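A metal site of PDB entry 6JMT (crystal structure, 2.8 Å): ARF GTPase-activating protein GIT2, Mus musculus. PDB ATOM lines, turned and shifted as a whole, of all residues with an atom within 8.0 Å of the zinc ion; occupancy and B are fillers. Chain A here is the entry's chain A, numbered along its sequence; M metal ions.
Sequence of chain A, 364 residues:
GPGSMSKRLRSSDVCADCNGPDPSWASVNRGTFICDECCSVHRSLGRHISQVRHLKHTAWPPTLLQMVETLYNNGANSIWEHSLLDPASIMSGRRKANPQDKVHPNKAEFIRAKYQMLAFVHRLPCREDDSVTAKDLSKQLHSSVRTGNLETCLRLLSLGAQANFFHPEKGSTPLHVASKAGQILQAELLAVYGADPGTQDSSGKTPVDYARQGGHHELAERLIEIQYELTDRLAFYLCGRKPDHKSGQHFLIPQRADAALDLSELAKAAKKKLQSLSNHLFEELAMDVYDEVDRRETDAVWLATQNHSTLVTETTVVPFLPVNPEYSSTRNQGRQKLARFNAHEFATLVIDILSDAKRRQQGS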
ATOM      1  N   VAL A  14      18.703  25.700  -7.074  1.00  0.00           N
ATOM      2  CA  VAL A  14      17.577  26.607  -7.078  1.00  0.00           C
ATOM      3  C   VAL A  14      16.343  26.073  -7.792  1.00  0.00           C
ATOM      4  O   VAL A  14      16.431  25.274  -8.723  1.00  0.00           O
ATOM      5  CB  VAL A  14      17.949  27.958  -7.715  1.00  0.00           C
ATOM      6  CG1 VAL A  14      18.865  28.734  -6.806  1.00  0.00           C
ATOM      7  CG2 VAL A  14      18.595  27.747  -9.061  1.00  0.00           C
ATOM      8  N   CYS A  15      15.202  26.536  -7.330  1.00  0.00           N
ATOM      9  CA  CYS A  15      13.933  26.292  -7.973  1.00  0.00           C
ATOM     10  C   CYS A  15      13.959  26.847  -9.376  1.00  0.00           C
ATOM     11  O   CYS A  15      14.366  27.986  -9.591  1.00  0.00           O
ATOM     12  CB  CYS A  15      12.813  26.936  -7.147  1.00  0.00           C
ATOM     13  SG  CYS A  15      11.161  26.595  -7.700  1.00  0.00           S
ATOM     14  N   ALA A  16      13.527  26.052 -10.350  1.00  0.00           N
ATOM     15  CA  ALA A  16      13.437  26.493 -11.743  1.00  0.00           C
ATOM     16  C   ALA A  16      12.358  27.549 -11.983  1.00  0.00           C
ATOM     17  O   ALA A  16      12.294  28.148 -13.062  1.00  0.00           O
ATOM     18  CB  ALA A  16      13.178  25.295 -12.656  1.00  0.00           C
ATOM     19  N   ASP A  17      11.488  27.763 -10.999  1.00  0.00           N
ATOM     20  CA  ASP A  17      10.304  28.583 -11.223  1.00  0.00           C
ATOM     21  C   ASP A  17      10.302  29.840 -10.386  1.00  0.00           C
ATOM     22  O   ASP A  17       9.582  30.783 -10.688  1.00  0.00           O
ATOM     23  CB  ASP A  17       9.038  27.796 -10.925  1.00  0.00           C
ATOM     24  CG  ASP A  17       8.847  26.612 -11.865  1.00  0.00           C
ATOM     25  OD1 ASP A  17       9.485  26.593 -12.947  1.00  0.00           O
ATOM     26  OD2 ASP A  17       8.068  25.685 -11.518  1.00  0.00           O
ATOM     27  N   CYS A  18      11.102  29.872  -9.324  1.00  0.00           N
ATOM     28  CA  CYS A  18      11.154  31.066  -8.489  1.00  0.00           C
ATOM     29  C   CYS A  18      12.551  31.405  -7.988  1.00  0.00           C
ATOM     30  O   CYS A  18      12.735  32.415  -7.308  1.00  0.00           O
ATOM     31  CB  CYS A  18      10.201  30.897  -7.300  1.00  0.00           C
ATOM     32  SG  CYS A  18      10.821  29.885  -5.935  1.00  0.00           S
ATOM     33  N   ASN A  19      13.486  30.536  -8.285  1.00  0.00           N
ATOM     34  CA  ASN A  19      14.850  30.768  -7.917  1.00  0.00           C
ATOM     35  C   ASN A  19      15.050  30.555  -6.458  1.00  0.00           C
ATOM     36  O   ASN A  19      16.042  30.938  -5.922  1.00  0.00           O
ATOM     37  CB  ASN A  19      15.210  32.162  -8.297  1.00  0.00           C
ATOM     38  CG  ASN A  19      15.822  32.232  -9.637  1.00  0.00           C
ATOM     39  OD1 ASN A  19      16.537  31.358 -10.033  1.00  0.00           O
ATOM     40  ND2 ASN A  19      15.567  33.297 -10.329  1.00  0.00           N
ATOM     41  N   GLY A  20      14.089  29.941  -5.821  1.00  0.00           N
ATOM     42  CA  GLY A  20      14.149  29.624  -4.418  1.00  0.00           C
ATOM     43  C   GLY A  20      15.151  28.547  -4.109  1.00  0.00           C
ATOM     44  O   GLY A  20      15.340  27.625  -4.879  1.00  0.00           O
ATOM     45  N   PRO A  21      15.786  28.684  -2.876  1.00  0.00           N
ATOM     46  CA  PRO A  21      16.915  27.781  -2.703  1.00  0.00           C
ATOM     47  C   PRO A  21      16.512  26.378  -2.369  1.00  0.00           C
ATOM     48  O   PRO A  21      15.419  26.134  -1.956  1.00  0.00           O
ATOM     49  CB  PRO A  21      17.675  28.387  -1.535  1.00  0.00           C
ATOM     50  CG  PRO A  21      16.605  28.793  -0.643  1.00  0.00           C
ATOM     51  CD  PRO A  21      15.649  29.475  -1.556  1.00  0.00           C
ATOM     52  N   PRO A  23      15.701  23.119  -3.624  1.00  0.00           N
ATOM     53  CA  PRO A  23      14.457  22.452  -4.065  1.00  0.00           C
ATOM     54  C   PRO A  23      14.275  20.957  -3.793  1.00  0.00           C
ATOM     55  O   PRO A  23      15.205  20.222  -3.820  1.00  0.00           O
ATOM     56  CB  PRO A  23      14.467  22.677  -5.563  1.00  0.00           C
ATOM     57  CG  PRO A  23      15.843  22.990  -5.906  1.00  0.00           C
ATOM     58  CD  PRO A  23      16.436  23.683  -4.738  1.00  0.00           C
ATOM     59  N   PHE A  33      14.021  20.997 -11.310  1.00  0.00           N
ATOM     60  CA  PHE A  33      13.783  20.815  -9.883  1.00  0.00           C
ATOM     61  C   PHE A  33      12.979  22.011  -9.404  1.00  0.00           C
ATOM     62  O   PHE A  33      13.228  23.137  -9.817  1.00  0.00           O
ATOM     63  CB  PHE A  33      15.066  20.702  -9.054  1.00  0.00           C
ATOM     64  CG  PHE A  33      15.902  19.468  -9.340  1.00  0.00           C
ATOM     65  CD1 PHE A  33      15.384  18.399 -10.058  1.00  0.00           C
ATOM     66  CD2 PHE A  33      17.212  19.384  -8.860  1.00  0.00           C
ATOM     67  CE1 PHE A  33      16.156  17.266 -10.309  1.00  0.00           C
ATOM     68  CE2 PHE A  33      17.997  18.280  -9.098  1.00  0.00           C
ATOM     69  CZ  PHE A  33      17.470  17.210  -9.821  1.00  0.00           C
ATOM     70  N   ILE A  34      12.005  21.788  -8.539  1.00  0.00           N
ATOM     71  CA  ILE A  34      11.211  22.875  -8.037  1.00  0.00           C
ATOM     72  C   ILE A  34      11.060  22.798  -6.515  1.00  0.00           C
ATOM     73  O   ILE A  34      11.297  21.734  -5.919  1.00  0.00           O
ATOM     74  CB  ILE A  34       9.829  22.873  -8.688  1.00  0.00           C
ATOM     75  CG1 ILE A  34       9.126  21.554  -8.404  1.00  0.00           C
ATOM     76  CG2 ILE A  34       9.966  23.090 -10.190  1.00  0.00           C
ATOM     77  CD1 ILE A  34       7.742  21.489  -8.949  1.00  0.00           C
ATOM     78  N   CYS A  35      10.681  23.915  -5.902  1.00  0.00           N
ATOM     79  CA  CYS A  35      10.447  23.948  -4.463  1.00  0.00           C
ATOM     80  C   CYS A  35       9.021  23.474  -4.119  1.00  0.00           C
ATOM     81  O   CYS A  35       8.207  23.239  -4.996  1.00  0.00           O
ATOM     82  CB  CYS A  35      10.655  25.351  -3.919  1.00  0.00           C
ATOM     83  SG  CYS A  35       9.340  26.456  -4.438  1.00  0.00           S
ATOM     84  N   ASP A  36       8.746  23.352  -2.833  1.00  0.00           N
ATOM     85  CA  ASP A  36       7.442  22.901  -2.378  1.00  0.00           C
ATOM     86  C   ASP A  36       6.271  23.727  -2.897  1.00  0.00           C
ATOM     87  O   ASP A  36       5.342  23.197  -3.502  1.00  0.00           O
ATOM     88  CB  ASP A  36       7.406  22.886  -0.852  1.00  0.00           C
ATOM     89  CG  ASP A  36       8.342  21.862  -0.269  1.00  0.00           C
ATOM     90  OD1 ASP A  36       8.024  20.656  -0.415  1.00  0.00           O
ATOM     91  OD2 ASP A  36       9.376  22.246   0.319  1.00  0.00           O
ATOM     92  N   GLU A  37       6.323  25.028  -2.646  1.00  0.00           N
ATOM     93  CA  GLU A  37       5.269  25.945  -3.083  1.00  0.00           C
ATOM     94  C   GLU A  37       4.985  25.824  -4.590  1.00  0.00           C
ATOM     95  O   GLU A  37       3.832  25.676  -5.016  1.00  0.00           O
ATOM     96  CB  GLU A  37       5.648  27.386  -2.752  1.00  0.00           C
ATOM     97  CG  GLU A  37       5.846  27.647  -1.284  1.00  0.00           C
ATOM     98  CD  GLU A  37       5.961  29.121  -0.994  1.00  0.00           C
ATOM     99  OE1 GLU A  37       5.810  29.914  -1.943  1.00  0.00           O
ATOM    100  OE2 GLU A  37       6.196  29.501   0.172  1.00  0.00           O
ATOM    101  N   CYS A  38       6.038  25.874  -5.395  1.00  0.00           N
ATOM    102  CA  CYS A  38       5.857  25.762  -6.818  1.00  0.00           C
ATOM    103  C   CYS A  38       5.332  24.379  -7.185  1.00  0.00           C
ATOM    104  O   CYS A  38       4.578  24.236  -8.158  1.00  0.00           O
ATOM    105  CB  CYS A  38       7.156  26.090  -7.547  1.00  0.00           C
ATOM    106  SG  CYS A  38       7.712  27.798  -7.270  1.00  0.00           S
ATOM    107  N   CYS A  39       5.697  23.372  -6.389  1.00  0.00           N
ATOM    108  CA  CYS A  39       5.206  22.027  -6.652  1.00  0.00           C
ATOM    109  C   CYS A  39       3.716  21.998  -6.437  1.00  0.00           C
ATOM    110  O   CYS A  39       3.008  21.404  -7.243  1.00  0.00           O
ATOM    111  CB  CYS A  39       5.880  20.984  -5.769  1.00  0.00           C
ATOM    112  SG  CYS A  39       5.305  19.236  -6.111  1.00  0.00           S
ATOM    113  N   HIS A  42       2.226  22.783  -9.373  1.00  0.00           N
ATOM    114  CA  HIS A  42       2.422  21.729 -10.372  1.00  0.00           C
ATOM    115  C   HIS A  42       1.378  20.620 -10.220  1.00  0.00           C
ATOM    116  O   HIS A  42       0.857  20.092 -11.210  1.00  0.00           O
ATOM    117  CB  HIS A  42       3.811  21.114 -10.265  1.00  0.00           C
ATOM    118  CG  HIS A  42       4.855  21.870 -11.011  1.00  0.00           C
ATOM    119  ND1 HIS A  42       5.543  21.324 -12.074  1.00  0.00           N
ATOM    120  CD2 HIS A  42       5.353  23.120 -10.850  1.00  0.00           C
ATOM    121  CE1 HIS A  42       6.408  22.214 -12.538  1.00  0.00           C
ATOM    122  NE2 HIS A  42       6.320  23.308 -11.805  1.00  0.00           N
ATOM    123  N   ALA A  97       8.838  34.790 -11.340  1.00  0.00           N
ATOM    124  CA  ALA A  97       8.591  34.937  -9.901  1.00  0.00           C
ATOM    125  C   ALA A  97       9.884  34.933  -9.071  1.00  0.00           C
ATOM    126  O   ALA A  97      10.917  34.435  -9.512  1.00  0.00           O
ATOM    127  CB  ALA A  97       7.658  33.845  -9.413  1.00  0.00           C
ATOM    128  N   ASN A  98       9.811  35.504  -7.873  1.00  0.00           N
ATOM    129  CA  ASN A  98      10.943  35.548  -6.936  1.00  0.00           C
ATOM    130  C   ASN A  98      10.577  34.764  -5.677  1.00  0.00           C
ATOM    131  O   ASN A  98       9.387  34.575  -5.395  1.00  0.00           O
ATOM    132  CB  ASN A  98      11.356  36.985  -6.581  1.00  0.00           C
ATOM    133  CG  ASN A  98      11.935  37.747  -7.765  1.00  0.00           C
ATOM    134  OD1 ASN A  98      13.056  37.495  -8.212  1.00  0.00           O
ATOM    135  ND2 ASN A  98      11.184  38.740  -8.240  1.00  0.00           N
ATOM    136  N   PRO A  99      11.578  34.265  -4.915  1.00  0.00           N
ATOM    137  CA  PRO A  99      11.263  33.313  -3.831  1.00  0.00           C
ATOM    138  C   PRO A  99      10.198  33.759  -2.825  1.00  0.00           C
ATOM    139  O   PRO A  99       9.430  32.937  -2.302  1.00  0.00           O
ATOM    140  CB  PRO A  99      12.603  33.152  -3.127  1.00  0.00           C
ATOM    141  CG  PRO A  99      13.618  33.438  -4.176  1.00  0.00           C
ATOM    142  CD  PRO A  99      13.024  34.521  -5.028  1.00  0.00           C
ATOM    143  N   LYS A 107       3.220  33.367  -8.006  1.00  0.00           N
ATOM    144  CA  LYS A 107       3.924  32.181  -8.467  1.00  0.00           C
ATOM    145  C   LYS A 107       3.022  31.347  -9.349  1.00  0.00           C
ATOM    146  O   LYS A 107       3.477  30.820 -10.354  1.00  0.00           O
ATOM    147  CB  LYS A 107       4.427  31.372  -7.295  1.00  0.00           C
ATOM    148  CG  LYS A 107       5.704  31.928  -6.716  1.00  0.00           C
ATOM    149  CD  LYS A 107       6.078  31.195  -5.441  1.00  0.00           C
ATOM    150  CE  LYS A 107       7.482  31.554  -4.981  1.00  0.00           C
ATOM    151  NZ  LYS A 107       7.886  30.802  -3.759  1.00  0.00           N
ATOM    152  N   ILE A 111       3.828  30.040 -13.218  1.00  0.00           N
ATOM    153  CA  ILE A 111       3.973  28.614 -13.476  1.00  0.00           C
ATOM    154  C   ILE A 111       3.005  28.161 -14.580  1.00  0.00           C
ATOM    155  O   ILE A 111       3.415  27.466 -15.503  1.00  0.00           O
ATOM    156  CB  ILE A 111       3.780  27.796 -12.173  1.00  0.00           C
ATOM    157  CG1 ILE A 111       4.863  28.179 -11.170  1.00  0.00           C
ATOM    158  CG2 ILE A 111       3.806  26.292 -12.424  1.00  0.00           C
ATOM    159  CD1 ILE A 111       4.824  27.380  -9.931  1.00  0.00           C
HETATM  160 ZN    ZN M   1       9.689  27.799  -6.347  1.00  0.00          ZN
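The side-chain sulfur (SG) of Cys 15 lies close to the backbone NH (N) of Asp 17, at 3.5 Å. O of Gly 20 is in hydrogen-bond range of N of Cys 15 (2.7 Å). N of Glu 37 sits close to SG of Cys 35 (3.8 Å). The side-chain sulfur (SG) of Cys 18 sits close to the side-chain amino group (NZ) of Lys 107 (3.8 Å). The side-chain sulfur of Cys 18 sits close to the backbone NH of Gly 20, at 3.3 Å.
Four residues have an atom within 4 Å of the zinc ion: Cys 15, Cys 18, Cys 35 and Cys 38. Along chain A the residues within 4 Å of the zinc ion span positions 15 to 38. The nearest printed residue that does not touch the zinc ion is Lys 107 (4.4 Å).
The zinc ion is bound by the side-chain sulfur (SG) of Cys 38 (2.2 Å), the side-chain sulfur (SG) of Cys 15 (2.3 Å), the side-chain sulfur (SG) of Cys 35 (2.4 Å) and the side-chain sulfur (SG) of Cys 18 (2.4 Å).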
